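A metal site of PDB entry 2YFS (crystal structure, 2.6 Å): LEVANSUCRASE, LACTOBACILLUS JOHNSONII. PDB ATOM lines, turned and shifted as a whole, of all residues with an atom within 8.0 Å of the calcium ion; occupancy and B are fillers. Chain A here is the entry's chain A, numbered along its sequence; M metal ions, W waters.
The calcium ion is bound by OD1 of Asn 174, water W1, OD2 of Asp 517, OG of Ser 524, water W2, O of Ile 519 and OD1 of Asp 517.
Merely in contact with the calcium ion: Gly 172 (3.9 Å).
Of the 19 residues printed, 5 come within 4 Å of the calcium ion.
The side-chain amide oxygen of Asn 174 sits close to the backbone carbonyl oxygen of Gly 172 (3.3 Å).
OG of Ser 523 sits at hydrogen-bond distance from ND2 of Asn 174, at 3.4 Å.
O of Asn 174 sits at hydrogen-bond distance from ND2 of Asn 514, at 2.9 Å.
OD1 of Asp 521 is in hydrogen-bond range of N of Ser 524.
Water W2 bridges the side-chain carboxylate (OD2) of Asp 521 and the backbone carbonyl oxygen (O) of Gly 172.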
ATOM      1  N   GLN A 148      19.814   0.569   3.957  1.00  0.00           N
ATOM      2  CA  GLN A 148      18.697  -0.005   3.176  1.00  0.00           C
ATOM      3  C   GLN A 148      17.418   0.117   4.042  1.00  0.00           C
ATOM      4  O   GLN A 148      17.466  -0.016   5.273  1.00  0.00           O
ATOM      5  CB  GLN A 148      18.958  -1.457   2.749  1.00  0.00           C
ATOM      6  CG  GLN A 148      19.347  -2.353   3.905  1.00  0.00           C
ATOM      7  CD  GLN A 148      19.651  -3.800   3.530  1.00  0.00           C
ATOM      8  OE1 GLN A 148      18.929  -4.407   2.747  1.00  0.00           O
ATOM      9  NE2 GLN A 148      20.688  -4.372   4.121  1.00  0.00           N
ATOM     10  N   TYR A 171      23.406  -0.657   4.424  1.00  0.00           N
ATOM     11  CA  TYR A 171      23.231  -1.148   3.076  1.00  0.00           C
ATOM     12  C   TYR A 171      24.175  -2.295   2.848  1.00  0.00           C
ATOM     13  O   TYR A 171      25.354  -2.209   3.210  1.00  0.00           O
ATOM     14  CB  TYR A 171      23.517  -0.074   2.025  1.00  0.00           C
ATOM     15  CG  TYR A 171      23.077  -0.491   0.645  1.00  0.00           C
ATOM     16  CD1 TYR A 171      21.769  -0.247   0.214  1.00  0.00           C
ATOM     17  CD2 TYR A 171      23.936  -1.148  -0.220  1.00  0.00           C
ATOM     18  CE1 TYR A 171      21.337  -0.630  -1.054  1.00  0.00           C
ATOM     19  CE2 TYR A 171      23.508  -1.549  -1.500  1.00  0.00           C
ATOM     20  CZ  TYR A 171      22.208  -1.268  -1.918  1.00  0.00           C
ATOM     21  OH  TYR A 171      21.752  -1.664  -3.165  1.00  0.00           O
ATOM     22  N   GLY A 172      23.647  -3.372   2.280  1.00  0.00           N
ATOM     23  CA  GLY A 172      24.455  -4.554   1.978  1.00  0.00           C
ATOM     24  C   GLY A 172      24.640  -5.524   3.121  1.00  0.00           C
ATOM     25  O   GLY A 172      25.032  -6.671   2.885  1.00  0.00           O
ATOM     26  N   ASP A 173      24.367  -5.092   4.359  1.00  0.00           N
ATOM     27  CA  ASP A 173      24.440  -5.971   5.550  1.00  0.00           C
ATOM     28  C   ASP A 173      23.481  -7.149   5.408  1.00  0.00           C
ATOM     29  O   ASP A 173      22.364  -6.973   4.943  1.00  0.00           O
ATOM     30  CB  ASP A 173      24.129  -5.146   6.794  1.00  0.00           C
ATOM     31  CG  ASP A 173      24.218  -5.960   8.094  1.00  0.00           C
ATOM     32  OD1 ASP A 173      23.637  -7.071   8.198  1.00  0.00           O
ATOM     33  OD2 ASP A 173      24.835  -5.454   9.069  1.00  0.00           O
ATOM     34  N   ASN A 174      23.921  -8.330   5.820  1.00  0.00           N
ATOM     35  CA  ASN A 174      23.183  -9.581   5.675  1.00  0.00           C
ATOM     36  C   ASN A 174      22.673 -10.166   6.991  1.00  0.00           C
ATOM     37  O   ASN A 174      21.995 -11.212   6.994  1.00  0.00           O
ATOM     38  CB  ASN A 174      24.063 -10.654   5.028  1.00  0.00           C
ATOM     39  CG  ASN A 174      24.534 -10.273   3.639  1.00  0.00           C
ATOM     40  OD1 ASN A 174      23.762  -9.749   2.828  1.00  0.00           O
ATOM     41  ND2 ASN A 174      25.790 -10.545   3.358  1.00  0.00           N
ATOM     42  N   ASP A 175      22.987  -9.534   8.107  1.00  0.00           N
ATOM     43  CA  ASP A 175      22.646 -10.098   9.394  1.00  0.00           C
ATOM     44  C   ASP A 175      21.184  -9.771   9.724  1.00  0.00           C
ATOM     45  O   ASP A 175      20.807  -8.610   9.908  1.00  0.00           O
ATOM     46  CB  ASP A 175      23.621  -9.616  10.482  1.00  0.00           C
ATOM     47  CG  ASP A 175      23.466 -10.394  11.783  1.00  0.00           C
ATOM     48  OD1 ASP A 175      22.505 -11.150  11.943  1.00  0.00           O
ATOM     49  OD2 ASP A 175      24.311 -10.240  12.681  1.00  0.00           O
ATOM     50  N   LEU A 472      16.060 -11.680  -7.370  1.00  0.00           N
ATOM     51  CA  LEU A 472      15.996 -12.138  -5.985  1.00  0.00           C
ATOM     52  C   LEU A 472      14.531 -12.245  -5.556  1.00  0.00           C
ATOM     53  O   LEU A 472      13.816 -11.248  -5.573  1.00  0.00           O
ATOM     54  CB  LEU A 472      16.730 -11.159  -5.072  1.00  0.00           C
ATOM     55  CG  LEU A 472      17.060 -11.652  -3.652  1.00  0.00           C
ATOM     56  CD1 LEU A 472      17.869 -12.950  -3.719  1.00  0.00           C
ATOM     57  CD2 LEU A 472      17.820 -10.599  -2.870  1.00  0.00           C
ATOM     58  N   THR A 513      19.781 -17.062   0.467  1.00  0.00           N
ATOM     59  CA  THR A 513      20.415 -16.102   1.368  1.00  0.00           C
ATOM     60  C   THR A 513      20.029 -16.309   2.826  1.00  0.00           C
ATOM     61  O   THR A 513      19.264 -17.188   3.137  1.00  0.00           O
ATOM     62  CB  THR A 513      20.012 -14.673   1.027  1.00  0.00           C
ATOM     63  OG1 THR A 513      18.611 -14.524   1.337  1.00  0.00           O
ATOM     64  CG2 THR A 513      20.312 -14.334  -0.455  1.00  0.00           C
ATOM     65  N   ASN A 514      20.587 -15.480   3.712  1.00  0.00           N
ATOM     66  CA  ASN A 514      20.123 -15.319   5.089  1.00  0.00           C
ATOM     67  C   ASN A 514      18.661 -14.832   5.091  1.00  0.00           C
ATOM     68  O   ASN A 514      18.186 -14.299   4.093  1.00  0.00           O
ATOM     69  CB  ASN A 514      20.972 -14.252   5.786  1.00  0.00           C
ATOM     70  CG  ASN A 514      22.299 -14.771   6.340  1.00  0.00           C
ATOM     71  OD1 ASN A 514      22.555 -15.972   6.362  1.00  0.00           O
ATOM     72  ND2 ASN A 514      23.132 -13.858   6.810  1.00  0.00           N
ATOM     73  N   GLY A 516      15.819 -12.364   5.337  1.00  0.00           N
ATOM     74  CA  GLY A 516      15.646 -10.939   5.246  1.00  0.00           C
ATOM     75  C   GLY A 516      16.656 -10.162   4.424  1.00  0.00           C
ATOM     76  O   GLY A 516      16.742  -8.939   4.547  1.00  0.00           O
ATOM     77  N   ASP A 517      17.400 -10.869   3.579  1.00  0.00           N
ATOM     78  CA  ASP A 517      18.303 -10.253   2.632  1.00  0.00           C
ATOM     79  C   ASP A 517      17.528  -9.810   1.381  1.00  0.00           C
ATOM     80  O   ASP A 517      16.924 -10.617   0.672  1.00  0.00           O
ATOM     81  CB  ASP A 517      19.381 -11.251   2.242  1.00  0.00           C
ATOM     82  CG  ASP A 517      20.614 -10.583   1.636  1.00  0.00           C
ATOM     83  OD1 ASP A 517      20.487  -9.474   1.103  1.00  0.00           O
ATOM     84  OD2 ASP A 517      21.716 -11.171   1.690  1.00  0.00           O
ATOM     85  N   TRP A 518      17.543  -8.505   1.132  1.00  0.00           N
ATOM     86  CA  TRP A 518      16.924  -7.909  -0.027  1.00  0.00           C
ATOM     87  C   TRP A 518      17.947  -7.616  -1.136  1.00  0.00           C
ATOM     88  O   TRP A 518      17.577  -7.171  -2.214  1.00  0.00           O
ATOM     89  CB  TRP A 518      16.240  -6.597   0.387  1.00  0.00           C
ATOM     90  CG  TRP A 518      15.180  -6.827   1.397  1.00  0.00           C
ATOM     91  CD1 TRP A 518      15.357  -6.942   2.747  1.00  0.00           C
ATOM     92  CD2 TRP A 518      13.788  -7.007   1.143  1.00  0.00           C
ATOM     93  NE1 TRP A 518      14.157  -7.181   3.345  1.00  0.00           N
ATOM     94  CE2 TRP A 518      13.172  -7.234   2.390  1.00  0.00           C
ATOM     95  CE3 TRP A 518      12.995  -7.003  -0.014  1.00  0.00           C
ATOM     96  CZ2 TRP A 518      11.782  -7.458   2.531  1.00  0.00           C
ATOM     97  CZ3 TRP A 518      11.602  -7.229   0.102  1.00  0.00           C
ATOM     98  CH2 TRP A 518      11.012  -7.448   1.374  1.00  0.00           C
ATOM     99  N   ILE A 519      19.226  -7.849  -0.871  1.00  0.00           N
ATOM    100  CA  ILE A 519      20.280  -7.426  -1.785  1.00  0.00           C
ATOM    101  C   ILE A 519      21.260  -8.553  -2.089  1.00  0.00           C
ATOM    102  O   ILE A 519      22.182  -8.793  -1.310  1.00  0.00           O
ATOM    103  CB  ILE A 519      21.060  -6.231  -1.200  1.00  0.00           C
ATOM    104  CG1 ILE A 519      20.131  -5.039  -0.984  1.00  0.00           C
ATOM    105  CG2 ILE A 519      22.234  -5.847  -2.130  1.00  0.00           C
ATOM    106  CD1 ILE A 519      20.659  -4.056   0.031  1.00  0.00           C
ATOM    107  N   TRP A 520      21.070  -9.228  -3.213  1.00  0.00           N
ATOM    108  CA  TRP A 520      22.022 -10.236  -3.658  1.00  0.00           C
ATOM    109  C   TRP A 520      23.349  -9.623  -4.068  1.00  0.00           C
ATOM    110  O   TRP A 520      23.405  -8.614  -4.784  1.00  0.00           O
ATOM    111  CB  TRP A 520      21.500 -11.075  -4.835  1.00  0.00           C
ATOM    112  CG  TRP A 520      22.479 -12.181  -5.141  1.00  0.00           C
ATOM    113  CD1 TRP A 520      23.564 -12.120  -5.994  1.00  0.00           C
ATOM    114  CD2 TRP A 520      22.513 -13.485  -4.555  1.00  0.00           C
ATOM    115  NE1 TRP A 520      24.247 -13.325  -5.979  1.00  0.00           N
ATOM    116  CE2 TRP A 520      23.611 -14.177  -5.116  1.00  0.00           C
ATOM    117  CE3 TRP A 520      21.688 -14.160  -3.634  1.00  0.00           C
ATOM    118  CZ2 TRP A 520      23.921 -15.481  -4.772  1.00  0.00           C
ATOM    119  CZ3 TRP A 520      22.005 -15.473  -3.298  1.00  0.00           C
ATOM    120  CH2 TRP A 520      23.111 -16.112  -3.864  1.00  0.00           C
ATOM    121  N   ASP A 521      24.424 -10.235  -3.570  1.00  0.00           N
ATOM    122  CA  ASP A 521      25.761 -10.069  -4.096  1.00  0.00           C
ATOM    123  C   ASP A 521      26.563 -11.312  -3.705  1.00  0.00           C
ATOM    124  O   ASP A 521      25.993 -12.271  -3.185  1.00  0.00           O
ATOM    125  CB  ASP A 521      26.407  -8.782  -3.576  1.00  0.00           C
ATOM    126  CG  ASP A 521      26.344  -8.668  -2.073  1.00  0.00           C
ATOM    127  OD1 ASP A 521      26.544  -9.672  -1.358  1.00  0.00           O
ATOM    128  OD2 ASP A 521      26.115  -7.522  -1.621  1.00  0.00           O
ATOM    129  N   ASP A 522      27.858 -11.302  -3.952  1.00  0.00           N
ATOM    130  CA  ASP A 522      28.645 -12.535  -3.762  1.00  0.00           C
ATOM    131  C   ASP A 522      28.731 -12.985  -2.300  1.00  0.00           C
ATOM    132  O   ASP A 522      28.680 -14.200  -2.012  1.00  0.00           O
ATOM    133  CB  ASP A 522      30.008 -12.510  -4.483  1.00  0.00           C
ATOM    134  CG  ASP A 522      30.383 -11.103  -5.003  1.00  0.00           C
ATOM    135  OD1 ASP A 522      29.626 -10.541  -5.868  1.00  0.00           O
ATOM    136  OD2 ASP A 522      31.453 -10.566  -4.576  1.00  0.00           O
ATOM    137  N   SER A 523      28.795 -12.020  -1.380  1.00  0.00           N
ATOM    138  CA  SER A 523      28.837 -12.321   0.052  1.00  0.00           C
ATOM    139  C   SER A 523      27.500 -12.831   0.605  1.00  0.00           C
ATOM    140  O   SER A 523      27.432 -13.268   1.750  1.00  0.00           O
ATOM    141  CB  SER A 523      29.273 -11.079   0.842  1.00  0.00           C
ATOM    142  OG  SER A 523      28.199 -10.138   0.964  1.00  0.00           O
ATOM    143  N   SER A 524      26.438 -12.803  -0.202  1.00  0.00           N
ATOM    144  CA  SER A 524      25.076 -13.045   0.279  1.00  0.00           C
ATOM    145  C   SER A 524      24.697 -14.496   0.439  1.00  0.00           C
ATOM    146  O   SER A 524      23.797 -14.806   1.226  1.00  0.00           O
ATOM    147  CB  SER A 524      24.070 -12.402  -0.650  1.00  0.00           C
ATOM    148  OG  SER A 524      23.847 -11.052  -0.319  1.00  0.00           O
ATOM    149  N   GLU A 525      25.315 -15.388  -0.330  1.00  0.00           N
ATOM    150  CA  GLU A 525      24.872 -16.775  -0.314  1.00  0.00           C
ATOM    151  C   GLU A 525      25.121 -17.454   1.004  1.00  0.00           C
ATOM    152  O   GLU A 525      26.190 -17.312   1.573  1.00  0.00           O
ATOM    153  CB  GLU A 525      25.494 -17.590  -1.426  1.00  0.00           C
ATOM    154  CG  GLU A 525      24.578 -18.729  -1.789  1.00  0.00           C
ATOM    155  CD  GLU A 525      25.244 -19.835  -2.562  1.00  0.00           C
ATOM    156  OE1 GLU A 525      26.256 -19.566  -3.259  1.00  0.00           O
ATOM    157  OE2 GLU A 525      24.720 -20.971  -2.480  1.00  0.00           O
HETATM  158 CA    CA M   1      22.907  -9.277   0.934  1.00  0.00          CA
HETATM  159  O   HOH W   1      22.190  -7.435   2.210  1.00  0.00           O
HETATM  160  O   HOH W   2      24.594  -7.685   0.454  1.00  0.00           O
